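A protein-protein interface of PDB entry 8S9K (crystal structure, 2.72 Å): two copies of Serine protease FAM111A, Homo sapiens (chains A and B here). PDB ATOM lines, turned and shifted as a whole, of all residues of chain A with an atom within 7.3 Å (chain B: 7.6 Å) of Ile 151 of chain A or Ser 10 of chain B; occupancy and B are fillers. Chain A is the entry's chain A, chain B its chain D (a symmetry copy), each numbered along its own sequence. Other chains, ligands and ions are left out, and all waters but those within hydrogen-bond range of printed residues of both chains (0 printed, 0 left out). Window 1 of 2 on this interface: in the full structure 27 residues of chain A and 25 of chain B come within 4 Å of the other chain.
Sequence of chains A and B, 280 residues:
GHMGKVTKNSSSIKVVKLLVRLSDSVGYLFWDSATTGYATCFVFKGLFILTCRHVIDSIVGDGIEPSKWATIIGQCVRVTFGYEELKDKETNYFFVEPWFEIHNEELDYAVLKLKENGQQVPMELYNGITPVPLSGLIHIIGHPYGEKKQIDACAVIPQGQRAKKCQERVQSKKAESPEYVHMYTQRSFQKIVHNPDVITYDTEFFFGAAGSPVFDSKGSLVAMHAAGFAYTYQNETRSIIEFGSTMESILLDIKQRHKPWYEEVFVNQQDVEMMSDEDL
The backbone carbonyl oxygen (O) of Gly 142 of chain A sits at hydrogen-bond distance from the backbone NH (N) of Gln 150 of chain A, at 2.9 Å.
Asn 9 of chain A touches its own counterpart, Asn 9 of chain B.
Val 16 of chain A touches its own counterpart, Val 16 of chain B.
Of the 22 pairs that touch across the chains among the printed residues, 2 have their exchanged pair printed and touching as well.
The side-chain amide nitrogen of Asn 9 of chain A sits close to the side-chain amide nitrogen of Asn 9 of chain B (3.4 Å).
The backbone carbonyl oxygen of Lys 149 of chain A lies within hydrogen-bond range of the backbone NH of Ile 13 of chain B (2.9 Å).
The backbone NH of Ile 151 of chain A sits at hydrogen-bond distance from the backbone carbonyl oxygen of Ser 11 of chain B.
The side-chain carboxylate of Glu 204 of chain A sits at hydrogen-bond distance from the backbone NH of Asn 9 of chain B (2.8 Å).
The side-chain carboxylate (OE2) of Glu 204 of chain A is in hydrogen-bond range of the side-chain hydroxyl (OG) of Ser 10 of chain B, 3.1 Å away.
Ile 151 of chain A touches just these residues of chain B: Ser 10 (3.6 Å), Ser 11 (3.0 Å), Ile 13 (3.7 Å) and Val 16 (3.8 Å).
Of chain A, only Gln 150 (3.7 Å), Ile 151 (3.6 Å), Asp 152 (3.9 Å), Glu 204 (3.1 Å) and Phe 205 (3.5 Å) come within 4 Å of Ser 10 of chain B.
Printed residues of chain B within 4 Å of Val 20 of chain A: Val 16 and Lys 17.
Printed residues of chain A within 4 Å of Lys 17 of chain B: Val 20 (3.7 Å).
The nearest residue of chain A that does not touch Ser 10 of chain B is Ala 153 of chain A (5.6 Å).
The nearest printed residue of chain B that does not touch Lys 149 of chain A is Ser 11 of chain B (4.7 Å).
Hydrophobic or aromatic side chains of chain B that line the printed part of chain A: Ile 13 and Val 16.
Printed residues of chain A that touch a printed residue of chain B: Asn 9, Val 16, Val 20, Ser 23, Lys 149, Gln 150, Ile 151, Asp 152, Glu 204 and Phe 205.
Hydrophobic or aromatic side chains of chain A that line the printed part of chain B: Val 16, Val 20, Ile 151 and Phe 205.
Along chain A the printed residues that touch a printed residue of chain B span positions 9 to 205.
Among the printed residues, 22 pairs touch across the chains.
Among the printed residues, merely in contact across the chains: Glu 204 of chain A with Lys 8 of chain B (3.2 Å), Gln 150 of chain A with Ser 11 of chain B (3.4 Å), Ser 23 of chain A with Ile 13 of chain B (3.5 Å), Lys 149 of chain A with Ser 12 of chain B (3.5 Å), Val 16 of chain A with Val 16 of chain B (3.5 Å), Val 20 of chain A with Val 16 of chain B (3.5 Å), Phe 205 of chain A with Ser 10 of chain B (3.5 Å), Ile 151 of chain A with Ser 10 of chain B (3.6 Å), Val 20 of chain A with Lys 17 of chain B (3.7 Å), Gln 150 of chain A with Ser 10 of chain B (3.7 Å), Ile 151 of chain A with Ile 13 of chain B (3.7 Å), Ile 151 of chain A with Val 16 of chain B (3.8 Å), Glu 204 of chain A with Thr 7 of chain B (3.8 Å), Asp 152 of chain A with Ser 10 of chain B (3.9 Å), Gln 150 of chain A with Lys 8 of chain B (3.9 Å), Gln 150 of chain A with Ile 13 of chain B (3.9 Å) and Gln 150 of chain A with Ser 12 of chain B (3.9 Å).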
ATOM      1  N   ASN A   9       0.091 -15.997  20.444  1.00  0.00           N
ATOM      2  CA  ASN A   9      -0.152 -17.234  19.710  1.00  0.00           C
ATOM      3  C   ASN A   9      -1.579 -17.732  19.939  1.00  0.00           C
ATOM      4  O   ASN A   9      -2.055 -18.632  19.244  1.00  0.00           O
ATOM      5  CB  ASN A   9       0.862 -18.305  20.119  1.00  0.00           C
ATOM      6  CG  ASN A   9       0.790 -19.542  19.247  1.00  0.00           C
ATOM      7  OD1 ASN A   9       1.385 -19.592  18.170  1.00  0.00           O
ATOM      8  ND2 ASN A   9       0.057 -20.549  19.707  1.00  0.00           N
ATOM      9  N   SER A  11      -5.754 -17.505  20.063  1.00  0.00           N
ATOM     10  CA  SER A  11      -6.773 -17.050  19.132  1.00  0.00           C
ATOM     11  C   SER A  11      -8.105 -16.906  19.855  1.00  0.00           C
ATOM     12  O   SER A  11      -8.325 -17.484  20.922  1.00  0.00           O
ATOM     13  CB  SER A  11      -6.926 -18.016  17.951  1.00  0.00           C
ATOM     14  OG  SER A  11      -5.668 -18.309  17.369  1.00  0.00           O
ATOM     15  N   VAL A  15     -12.908 -16.696  15.848  1.00  0.00           N
ATOM     16  CA  VAL A  15     -12.079 -17.022  14.690  1.00  0.00           C
ATOM     17  C   VAL A  15     -11.890 -18.529  14.570  1.00  0.00           C
ATOM     18  O   VAL A  15     -11.904 -19.086  13.466  1.00  0.00           O
ATOM     19  CB  VAL A  15     -10.730 -16.284  14.772  1.00  0.00           C
ATOM     20  CG1 VAL A  15      -9.803 -16.744  13.657  1.00  0.00           C
ATOM     21  CG2 VAL A  15     -10.944 -14.779  14.699  1.00  0.00           C
ATOM     22  N   VAL A  16     -11.724 -19.217  15.701  1.00  0.00           N
ATOM     23  CA  VAL A  16     -11.514 -20.661  15.652  1.00  0.00           C
ATOM     24  C   VAL A  16     -12.796 -21.384  15.249  1.00  0.00           C
ATOM     25  O   VAL A  16     -12.750 -22.410  14.558  1.00  0.00           O
ATOM     26  CB  VAL A  16     -10.970 -21.160  17.002  1.00  0.00           C
ATOM     27  CG1 VAL A  16     -10.706 -22.643  16.945  1.00  0.00           C
ATOM     28  CG2 VAL A  16      -9.697 -20.412  17.366  1.00  0.00           C
ATOM     29  N   LEU A  19     -12.736 -21.153  11.657  1.00  0.00           N
ATOM     30  CA  LEU A  19     -11.706 -21.993  11.054  1.00  0.00           C
ATOM     31  C   LEU A  19     -12.118 -23.461  11.030  1.00  0.00           C
ATOM     32  O   LEU A  19     -11.799 -24.179  10.077  1.00  0.00           O
ATOM     33  CB  LEU A  19     -10.385 -21.822  11.801  1.00  0.00           C
ATOM     34  CG  LEU A  19      -9.642 -20.500  11.601  1.00  0.00           C
ATOM     35  CD1 LEU A  19      -8.481 -20.383  12.573  1.00  0.00           C
ATOM     36  CD2 LEU A  19      -9.152 -20.386  10.168  1.00  0.00           C
ATOM     37  N   VAL A  20     -12.814 -23.934  12.066  1.00  0.00           N
ATOM     38  CA  VAL A  20     -13.202 -25.343  12.062  1.00  0.00           C
ATOM     39  C   VAL A  20     -14.265 -25.607  11.004  1.00  0.00           C
ATOM     40  O   VAL A  20     -14.314 -26.700  10.428  1.00  0.00           O
ATOM     41  CB  VAL A  20     -13.666 -25.804  13.456  1.00  0.00           C
ATOM     42  CG1 VAL A  20     -12.486 -25.859  14.405  1.00  0.00           C
ATOM     43  CG2 VAL A  20     -14.760 -24.895  13.993  1.00  0.00           C
ATOM     44  N   SER A  23     -12.354 -25.787   7.765  1.00  0.00           N
ATOM     45  CA  SER A  23     -11.511 -26.971   7.624  1.00  0.00           C
ATOM     46  C   SER A  23     -12.202 -28.086   6.852  1.00  0.00           C
ATOM     47  O   SER A  23     -11.520 -28.949   6.291  1.00  0.00           O
ATOM     48  CB  SER A  23     -11.082 -27.488   8.999  1.00  0.00           C
ATOM     49  OG  SER A  23     -12.165 -28.098   9.677  1.00  0.00           O
ATOM     50  N   ILE A 138      -1.000 -16.317  11.942  1.00  0.00           N
ATOM     51  CA  ILE A 138      -1.705 -16.987  10.857  1.00  0.00           C
ATOM     52  C   ILE A 138      -2.125 -18.374  11.328  1.00  0.00           C
ATOM     53  O   ILE A 138      -1.696 -18.858  12.375  1.00  0.00           O
ATOM     54  CB  ILE A 138      -0.860 -17.088   9.569  1.00  0.00           C
ATOM     55  CG1 ILE A 138       0.550 -17.588   9.891  1.00  0.00           C
ATOM     56  CG2 ILE A 138      -0.839 -15.755   8.838  1.00  0.00           C
ATOM     57  CD1 ILE A 138       1.402 -17.815   8.669  1.00  0.00           C
ATOM     58  N   HIS A 139      -2.971 -19.017  10.524  1.00  0.00           N
ATOM     59  CA  HIS A 139      -3.477 -20.352  10.825  1.00  0.00           C
ATOM     60  C   HIS A 139      -3.366 -21.217   9.580  1.00  0.00           C
ATOM     61  O   HIS A 139      -3.932 -20.880   8.536  1.00  0.00           O
ATOM     62  CB  HIS A 139      -4.931 -20.297  11.307  1.00  0.00           C
ATOM     63  CG  HIS A 139      -5.132 -19.472  12.542  1.00  0.00           C
ATOM     64  ND1 HIS A 139      -5.273 -18.102  12.509  1.00  0.00           N
ATOM     65  CD2 HIS A 139      -5.223 -19.828  13.846  1.00  0.00           C
ATOM     66  CE1 HIS A 139      -5.440 -17.647  13.737  1.00  0.00           C
ATOM     67  NE2 HIS A 139      -5.414 -18.674  14.568  1.00  0.00           N
ATOM     68  N   ILE A 140      -2.649 -22.332   9.689  1.00  0.00           N
ATOM     69  CA  ILE A 140      -2.477 -23.275   8.589  1.00  0.00           C
ATOM     70  C   ILE A 140      -3.300 -24.518   8.893  1.00  0.00           C
ATOM     71  O   ILE A 140      -3.213 -25.068   9.997  1.00  0.00           O
ATOM     72  CB  ILE A 140      -0.999 -23.642   8.382  1.00  0.00           C
ATOM     73  CG1 ILE A 140      -0.138 -22.379   8.338  1.00  0.00           C
ATOM     74  CG2 ILE A 140      -0.828 -24.458   7.108  1.00  0.00           C
ATOM     75  CD1 ILE A 140       1.343 -22.656   8.225  1.00  0.00           C
ATOM     76  N   ILE A 141      -4.095 -24.963   7.920  1.00  0.00           N
ATOM     77  CA  ILE A 141      -4.906 -26.170   8.082  1.00  0.00           C
ATOM     78  C   ILE A 141      -4.494 -27.176   7.019  1.00  0.00           C
ATOM     79  O   ILE A 141      -4.542 -26.871   5.821  1.00  0.00           O
ATOM     80  CB  ILE A 141      -6.412 -25.876   7.999  1.00  0.00           C
ATOM     81  CG1 ILE A 141      -6.831 -24.889   9.087  1.00  0.00           C
ATOM     82  CG2 ILE A 141      -7.210 -27.165   8.140  1.00  0.00           C
ATOM     83  CD1 ILE A 141      -8.328 -24.678   9.167  1.00  0.00           C
ATOM     84  N   GLY A 142      -4.109 -28.373   7.447  1.00  0.00           N
ATOM     85  CA  GLY A 142      -3.675 -29.359   6.479  1.00  0.00           C
ATOM     86  C   GLY A 142      -3.474 -30.725   7.095  1.00  0.00           C
ATOM     87  O   GLY A 142      -3.916 -30.998   8.211  1.00  0.00           O
ATOM     88  N   PRO A 144      -0.292 -32.651   7.770  1.00  0.00           N
ATOM     89  CA  PRO A 144       1.161 -32.856   7.846  1.00  0.00           C
ATOM     90  C   PRO A 144       1.501 -34.307   8.145  1.00  0.00           C
ATOM     91  O   PRO A 144       0.789 -34.987   8.888  1.00  0.00           O
ATOM     92  CB  PRO A 144       1.588 -31.929   8.989  1.00  0.00           C
ATOM     93  CG  PRO A 144       0.373 -31.824   9.843  1.00  0.00           C
ATOM     94  CD  PRO A 144      -0.791 -31.841   8.896  1.00  0.00           C
ATOM     95  N   GLU A 147      -0.916 -37.273   8.221  1.00  0.00           N
ATOM     96  CA  GLU A 147      -1.720 -37.612   9.382  1.00  0.00           C
ATOM     97  C   GLU A 147      -3.118 -37.015   9.252  1.00  0.00           C
ATOM     98  O   GLU A 147      -3.482 -36.418   8.235  1.00  0.00           O
ATOM     99  CB  GLU A 147      -1.030 -37.129  10.654  1.00  0.00           C
ATOM    100  CG  GLU A 147       0.369 -37.682  10.849  1.00  0.00           C
ATOM    101  CD  GLU A 147       1.120 -36.985  11.964  1.00  0.00           C
ATOM    102  OE1 GLU A 147       0.641 -35.931  12.431  1.00  0.00           O
ATOM    103  OE2 GLU A 147       2.188 -37.487  12.374  1.00  0.00           O
ATOM    104  N   LYS A 148      -3.915 -37.185  10.304  1.00  0.00           N
ATOM    105  CA  LYS A 148      -5.246 -36.602  10.352  1.00  0.00           C
ATOM    106  C   LYS A 148      -5.168 -35.081  10.236  1.00  0.00           C
ATOM    107  O   LYS A 148      -4.117 -34.468  10.444  1.00  0.00           O
ATOM    108  CB  LYS A 148      -5.951 -37.001  11.648  1.00  0.00           C
ATOM    109  CG  LYS A 148      -5.092 -36.813  12.886  1.00  0.00           C
ATOM    110  CD  LYS A 148      -5.773 -37.364  14.127  1.00  0.00           C
ATOM    111  CE  LYS A 148      -4.856 -37.274  15.339  1.00  0.00           C
ATOM    112  NZ  LYS A 148      -5.499 -37.819  16.567  1.00  0.00           N
ATOM    113  N   LYS A 149      -6.304 -34.475   9.895  1.00  0.00           N
ATOM    114  CA  LYS A 149      -6.347 -33.038   9.657  1.00  0.00           C
ATOM    115  C   LYS A 149      -6.008 -32.271  10.928  1.00  0.00           C
ATOM    116  O   LYS A 149      -6.520 -32.572  12.010  1.00  0.00           O
ATOM    117  CB  LYS A 149      -7.726 -32.634   9.141  1.00  0.00           C
ATOM    118  CG  LYS A 149      -7.756 -31.292   8.440  1.00  0.00           C
ATOM    119  CD  LYS A 149      -9.159 -30.952   7.977  1.00  0.00           C
ATOM    120  CE  LYS A 149      -9.723 -32.042   7.088  1.00  0.00           C
ATOM    121  NZ  LYS A 149     -11.098 -31.712   6.622  1.00  0.00           N
ATOM    122  N   GLN A 150      -5.133 -31.278  10.790  1.00  0.00           N
ATOM    123  CA  GLN A 150      -4.632 -30.509  11.917  1.00  0.00           C
ATOM    124  C   GLN A 150      -4.591 -29.034  11.544  1.00  0.00           C
ATOM    125  O   GLN A 150      -4.574 -28.663  10.363  1.00  0.00           O
ATOM    126  CB  GLN A 150      -3.235 -30.981  12.348  1.00  0.00           C
ATOM    127  CG  GLN A 150      -3.174 -32.427  12.815  1.00  0.00           C
ATOM    128  CD  GLN A 150      -1.751 -32.931  12.978  1.00  0.00           C
ATOM    129  OE1 GLN A 150      -0.885 -32.229  13.502  1.00  0.00           O
ATOM    130  NE2 GLN A 150      -1.501 -34.152  12.522  1.00  0.00           N
ATOM    131  N   ILE A 151      -4.576 -28.195  12.578  1.00  0.00           N
ATOM    132  CA  ILE A 151      -4.507 -26.747  12.436  1.00  0.00           C
ATOM    133  C   ILE A 151      -3.399 -26.227  13.342  1.00  0.00           C
ATOM    134  O   ILE A 151      -3.246 -26.684  14.479  1.00  0.00           O
ATOM    135  CB  ILE A 151      -5.858 -26.075  12.770  1.00  0.00           C
ATOM    136  CG1 ILE A 151      -5.744 -24.551  12.677  1.00  0.00           C
ATOM    137  CG2 ILE A 151      -6.359 -26.509  14.141  1.00  0.00           C
ATOM    138  CD1 ILE A 151      -7.017 -23.821  13.041  1.00  0.00           C
ATOM    139  N   ASP A 152      -2.615 -25.282  12.826  1.00  0.00           N
ATOM    140  CA  ASP A 152      -1.491 -24.714  13.557  1.00  0.00           C
ATOM    141  C   ASP A 152      -1.566 -23.196  13.518  1.00  0.00           C
ATOM    142  O   ASP A 152      -1.830 -22.603  12.466  1.00  0.00           O
ATOM    143  CB  ASP A 152      -0.150 -25.183  12.974  1.00  0.00           C
ATOM    144  CG  ASP A 152       1.033 -24.805  13.847  1.00  0.00           C
ATOM    145  OD1 ASP A 152       0.816 -24.374  15.001  1.00  0.00           O
ATOM    146  OD2 ASP A 152       2.184 -24.937  13.381  1.00  0.00           O
ATOM    147  N   ALA A 153      -1.337 -22.573  14.673  1.00  0.00           N
ATOM    148  CA  ALA A 153      -1.220 -21.126  14.792  1.00  0.00           C
ATOM    149  C   ALA A 153       0.257 -20.760  14.716  1.00  0.00           C
ATOM    150  O   ALA A 153       1.057 -21.224  15.535  1.00  0.00           O
ATOM    151  CB  ALA A 153      -1.839 -20.630  16.098  1.00  0.00           C
ATOM    152  N   CYS A 154       0.614 -19.928  13.740  1.00  0.00           N
ATOM    153  CA  CYS A 154       2.005 -19.708  13.381  1.00  0.00           C
ATOM    154  C   CYS A 154       2.341 -18.224  13.369  1.00  0.00           C
ATOM    155  O   CYS A 154       1.477 -17.363  13.172  1.00  0.00           O
ATOM    156  CB  CYS A 154       2.326 -20.313  12.010  1.00  0.00           C
ATOM    157  SG  CYS A 154       1.679 -21.974  11.790  1.00  0.00           S
ATOM    158  N   THR A 203       6.340 -22.720  11.262  1.00  0.00           N
ATOM    159  CA  THR A 203       5.264 -23.667  11.509  1.00  0.00           C
ATOM    160  C   THR A 203       5.840 -25.048  11.790  1.00  0.00           C
ATOM    161  O   THR A 203       7.019 -25.323  11.548  1.00  0.00           O
ATOM    162  CB  THR A 203       4.295 -23.748  10.322  1.00  0.00           C
ATOM    163  OG1 THR A 203       3.184 -24.583  10.670  1.00  0.00           O
ATOM    164  CG2 THR A 203       4.989 -24.337   9.105  1.00  0.00           C
ATOM    165  N   GLU A 204       4.978 -25.923  12.307  1.00  0.00           N
ATOM    166  CA  GLU A 204       5.303 -27.329  12.500  1.00  0.00           C
ATOM    167  C   GLU A 204       4.831 -28.204  11.349  1.00  0.00           C
ATOM    168  O   GLU A 204       5.161 -29.394  11.317  1.00  0.00           O
ATOM    169  CB  GLU A 204       4.693 -27.834  13.811  1.00  0.00           C
ATOM    170  CG  GLU A 204       5.178 -27.082  15.035  1.00  0.00           C
ATOM    171  CD  GLU A 204       4.217 -27.184  16.199  1.00  0.00           C
ATOM    172  OE1 GLU A 204       4.520 -26.621  17.273  1.00  0.00           O
ATOM    173  OE2 GLU A 204       3.155 -27.823  16.038  1.00  0.00           O
ATOM    174  N   PHE A 205       4.075 -27.645  10.407  1.00  0.00           N
ATOM    175  CA  PHE A 205       3.573 -28.382   9.248  1.00  0.00           C
ATOM    176  C   PHE A 205       4.546 -28.286   8.077  1.00  0.00           C
ATOM    177  O   PHE A 205       4.162 -27.990   6.947  1.00  0.00           O
ATOM    178  CB  PHE A 205       2.195 -27.865   8.849  1.00  0.00           C
ATOM    179  CG  PHE A 205       1.124 -28.087   9.884  1.00  0.00           C
ATOM    180  CD1 PHE A 205       1.384 -28.791  11.051  1.00  0.00           C
ATOM    181  CD2 PHE A 205      -0.156 -27.596   9.680  1.00  0.00           C
ATOM    182  CE1 PHE A 205       0.395 -28.992  11.995  1.00  0.00           C
ATOM    183  CE2 PHE A 205      -1.150 -27.794  10.619  1.00  0.00           C
ATOM    184  CZ  PHE A 205      -0.873 -28.493  11.777  1.00  0.00           C
ATOM    185  N   PHE A 215      -4.602 -18.968   6.522  1.00  0.00           N
ATOM    186  CA  PHE A 215      -5.553 -17.896   6.772  1.00  0.00           C
ATOM    187  C   PHE A 215      -4.935 -16.867   7.710  1.00  0.00           C
ATOM    188  O   PHE A 215      -4.059 -17.192   8.519  1.00  0.00           O
ATOM    189  CB  PHE A 215      -6.845 -18.436   7.399  1.00  0.00           C
ATOM    190  CG  PHE A 215      -7.392 -19.667   6.724  1.00  0.00           C
ATOM    191  CD1 PHE A 215      -6.894 -20.926   7.028  1.00  0.00           C
ATOM    192  CD2 PHE A 215      -8.419 -19.565   5.798  1.00  0.00           C
ATOM    193  CE1 PHE A 215      -7.398 -22.057   6.408  1.00  0.00           C
ATOM    194  CE2 PHE A 215      -8.927 -20.691   5.178  1.00  0.00           C
ATOM    195  CZ  PHE A 215      -8.415 -21.939   5.484  1.00  0.00           C
ATOM    196  N   THR B   7       7.763 -28.250  22.308  1.00  0.00           N
ATOM    197  CA  THR B   7       6.619 -29.146  22.257  1.00  0.00           C
ATOM    198  C   THR B   7       5.664 -28.695  21.154  1.00  0.00           C
ATOM    199  O   THR B   7       5.539 -27.502  20.868  1.00  0.00           O
ATOM    200  CB  THR B   7       5.889 -29.176  23.605  1.00  0.00           C
ATOM    201  OG1 THR B   7       6.840 -29.357  24.662  1.00  0.00           O
ATOM    202  CG2 THR B   7       4.875 -30.315  23.653  1.00  0.00           C
ATOM    203  N   LYS B   8       4.998 -29.664  20.531  1.00  0.00           N
ATOM    204  CA  LYS B   8       4.101 -29.364  19.421  1.00  0.00           C
ATOM    205  C   LYS B   8       2.915 -28.539  19.910  1.00  0.00           C
ATOM    206  O   LYS B   8       2.184 -28.958  20.813  1.00  0.00           O
ATOM    207  CB  LYS B   8       3.622 -30.654  18.757  1.00  0.00           C
ATOM    208  CG  LYS B   8       3.928 -30.719  17.266  1.00  0.00           C
ATOM    209  CD  LYS B   8       3.266 -31.913  16.596  1.00  0.00           C
ATOM    210  CE  LYS B   8       3.524 -31.908  15.096  1.00  0.00           C
ATOM    211  NZ  LYS B   8       2.820 -33.016  14.393  1.00  0.00           N
ATOM    212  N   ASN B   9       2.732 -27.361  19.311  1.00  0.00           N
ATOM    213  CA  ASN B   9       1.621 -26.478  19.636  1.00  0.00           C
ATOM    214  C   ASN B   9       0.364 -26.798  18.839  1.00  0.00           C
ATOM    215  O   ASN B   9      -0.740 -26.452  19.277  1.00  0.00           O
ATOM    216  CB  ASN B   9       2.032 -25.020  19.389  1.00  0.00           C
ATOM    217  CG  ASN B   9       1.208 -24.025  20.191  1.00  0.00           C
ATOM    218  OD1 ASN B   9      -0.020 -24.048  20.169  1.00  0.00           O
ATOM    219  ND2 ASN B   9       1.892 -23.136  20.903  1.00  0.00           N
ATOM    220  N   SER B  10       0.501 -27.465  17.697  1.00  0.00           N
ATOM    221  CA  SER B  10      -0.639 -27.722  16.829  1.00  0.00           C
ATOM    222  C   SER B  10      -1.559 -28.787  17.419  1.00  0.00           C
ATOM    223  O   SER B  10      -1.132 -29.665  18.176  1.00  0.00           O
ATOM    224  CB  SER B  10      -0.163 -28.163  15.446  1.00  0.00           C
ATOM    225  OG  SER B  10       0.507 -29.410  15.516  1.00  0.00           O
ATOM    226  N   SER B  11      -2.834 -28.705  17.050  1.00  0.00           N
ATOM    227  CA  SER B  11      -3.850 -29.644  17.493  1.00  0.00           C
ATOM    228  C   SER B  11      -4.587 -30.207  16.284  1.00  0.00           C
ATOM    229  O   SER B  11      -4.541 -29.648  15.185  1.00  0.00           O
ATOM    230  CB  SER B  11      -4.850 -28.978  18.447  1.00  0.00           C
ATOM    231  OG  SER B  11      -4.174 -28.263  19.466  1.00  0.00           O
ATOM    232  N   SER B  12      -5.270 -31.327  16.498  1.00  0.00           N
ATOM    233  CA  SER B  12      -6.067 -31.922  15.441  1.00  0.00           C
ATOM    234  C   SER B  12      -7.418 -31.221  15.341  1.00  0.00           C
ATOM    235  O   SER B  12      -7.905 -30.616  16.298  1.00  0.00           O
ATOM    236  CB  SER B  12      -6.273 -33.416  15.690  1.00  0.00           C
ATOM    237  OG  SER B  12      -7.110 -33.627  16.815  1.00  0.00           O
ATOM    238  N   ILE B  13      -8.027 -31.319  14.158  1.00  0.00           N
ATOM    239  CA  ILE B  13      -9.302 -30.650  13.917  1.00  0.00           C
ATOM    240  C   ILE B  13     -10.399 -31.233  14.796  1.00  0.00           C
ATOM    241  O   ILE B  13     -11.293 -30.509  15.248  1.00  0.00           O
ATOM    242  CB  ILE B  13      -9.662 -30.727  12.421  1.00  0.00           C
ATOM    243  CG1 ILE B  13      -8.706 -29.855  11.608  1.00  0.00           C
ATOM    244  CG2 ILE B  13     -11.094 -30.290  12.181  1.00  0.00           C
ATOM    245  CD1 ILE B  13      -8.756 -28.393  11.981  1.00  0.00           C
ATOM    246  N   LYS B  14     -10.345 -32.539  15.068  1.00  0.00           N
ATOM    247  CA  LYS B  14     -11.353 -33.162  15.921  1.00  0.00           C
ATOM    248  C   LYS B  14     -11.327 -32.570  17.326  1.00  0.00           C
ATOM    249  O   LYS B  14     -12.371 -32.199  17.882  1.00  0.00           O
ATOM    250  CB  LYS B  14     -11.132 -34.675  15.966  1.00  0.00           C
ATOM    251  CG  LYS B  14     -12.088 -35.405  16.888  1.00  0.00           C
ATOM    252  CD  LYS B  14     -11.704 -36.864  17.067  1.00  0.00           C
ATOM    253  CE  LYS B  14     -12.641 -37.548  18.055  1.00  0.00           C
ATOM    254  NZ  LYS B  14     -12.201 -38.930  18.395  1.00  0.00           N
ATOM    255  N   VAL B  16     -10.083 -29.696  18.228  1.00  0.00           N
ATOM    256  CA  VAL B  16     -10.428 -28.278  18.203  1.00  0.00           C
ATOM    257  C   VAL B  16     -11.938 -28.092  18.074  1.00  0.00           C
ATOM    258  O   VAL B  16     -12.514 -27.170  18.664  1.00  0.00           O
ATOM    259  CB  VAL B  16      -9.658 -27.562  17.079  1.00  0.00           C
ATOM    260  CG1 VAL B  16     -10.079 -26.113  16.995  1.00  0.00           C
ATOM    261  CG2 VAL B  16      -8.164 -27.655  17.329  1.00  0.00           C
ATOM    262  N   LYS B  17     -12.605 -28.965  17.313  1.00  0.00           N
ATOM    263  CA  LYS B  17     -14.063 -28.915  17.242  1.00  0.00           C
ATOM    264  C   LYS B  17     -14.687 -29.250  18.590  1.00  0.00           C
ATOM    265  O   LYS B  17     -15.658 -28.609  19.020  1.00  0.00           O
ATOM    266  CB  LYS B  17     -14.575 -29.871  16.167  1.00  0.00           C
ATOM    267  CG  LYS B  17     -14.357 -29.394  14.739  1.00  0.00           C
ATOM    268  CD  LYS B  17     -14.977 -30.360  13.747  1.00  0.00           C
ATOM    269  CE  LYS B  17     -14.807 -29.876  12.321  1.00  0.00           C
ATOM    270  NZ  LYS B  17     -15.325 -30.870  11.337  1.00  0.00           N
ATOM    271  N   LEU B 137       0.882 -31.205  25.670  1.00  0.00           N
ATOM    272  CA  LEU B 137       0.125 -30.028  25.277  1.00  0.00           C
ATOM    273  C   LEU B 137      -1.208 -30.000  26.009  1.00  0.00           C
ATOM    274  O   LEU B 137      -1.826 -31.046  26.228  1.00  0.00           O
ATOM    275  CB  LEU B 137      -0.105 -30.020  23.764  1.00  0.00           C
ATOM    276  CG  LEU B 137      -0.810 -28.816  23.137  1.00  0.00           C
ATOM    277  CD1 LEU B 137       0.116 -27.611  23.103  1.00  0.00           C
ATOM    278  CD2 LEU B 137      -1.299 -29.167  21.743  1.00  0.00           C
ATOM    279  N   HIS B 139      -4.886 -27.180  26.633  1.00  0.00           N
ATOM    280  CA  HIS B 139      -5.657 -26.070  26.093  1.00  0.00           C
ATOM    281  C   HIS B 139      -6.360 -25.346  27.230  1.00  0.00           C
ATOM    282  O   HIS B 139      -6.970 -25.982  28.091  1.00  0.00           O
ATOM    283  CB  HIS B 139      -6.685 -26.557  25.066  1.00  0.00           C
ATOM    284  CG  HIS B 139      -6.085 -27.300  23.913  1.00  0.00           C
ATOM    285  ND1 HIS B 139      -5.726 -28.628  23.990  1.00  0.00           N
ATOM    286  CD2 HIS B 139      -5.792 -26.903  22.652  1.00  0.00           C
ATOM    287  CE1 HIS B 139      -5.234 -29.017  22.826  1.00  0.00           C
ATOM    288  NE2 HIS B 139      -5.264 -27.989  21.998  1.00  0.00           N
ATOM    289  N   ALA B 153      -3.271 -22.939  23.258  1.00  0.00           N
ATOM    290  CA  ALA B 153      -2.600 -24.226  23.378  1.00  0.00           C
ATOM    291  C   ALA B 153      -1.227 -24.003  24.000  1.00  0.00           C
ATOM    292  O   ALA B 153      -0.401 -23.267  23.449  1.00  0.00           O
ATOM    293  CB  ALA B 153      -2.477 -24.910  22.016  1.00  0.00           C
ATOM    294  N   SER B 217      -4.592 -32.869  25.902  1.00  0.00           N
ATOM    295  CA  SER B 217      -4.407 -32.862  24.456  1.00  0.00           C
ATOM    296  C   SER B 217      -5.568 -33.514  23.717  1.00  0.00           C
ATOM    297  O   SER B 217      -5.774 -33.221  22.534  1.00  0.00           O
ATOM    298  CB  SER B 217      -3.096 -33.560  24.094  1.00  0.00           C
ATOM    299  OG  SER B 217      -3.015 -34.841  24.695  1.00  0.00           O
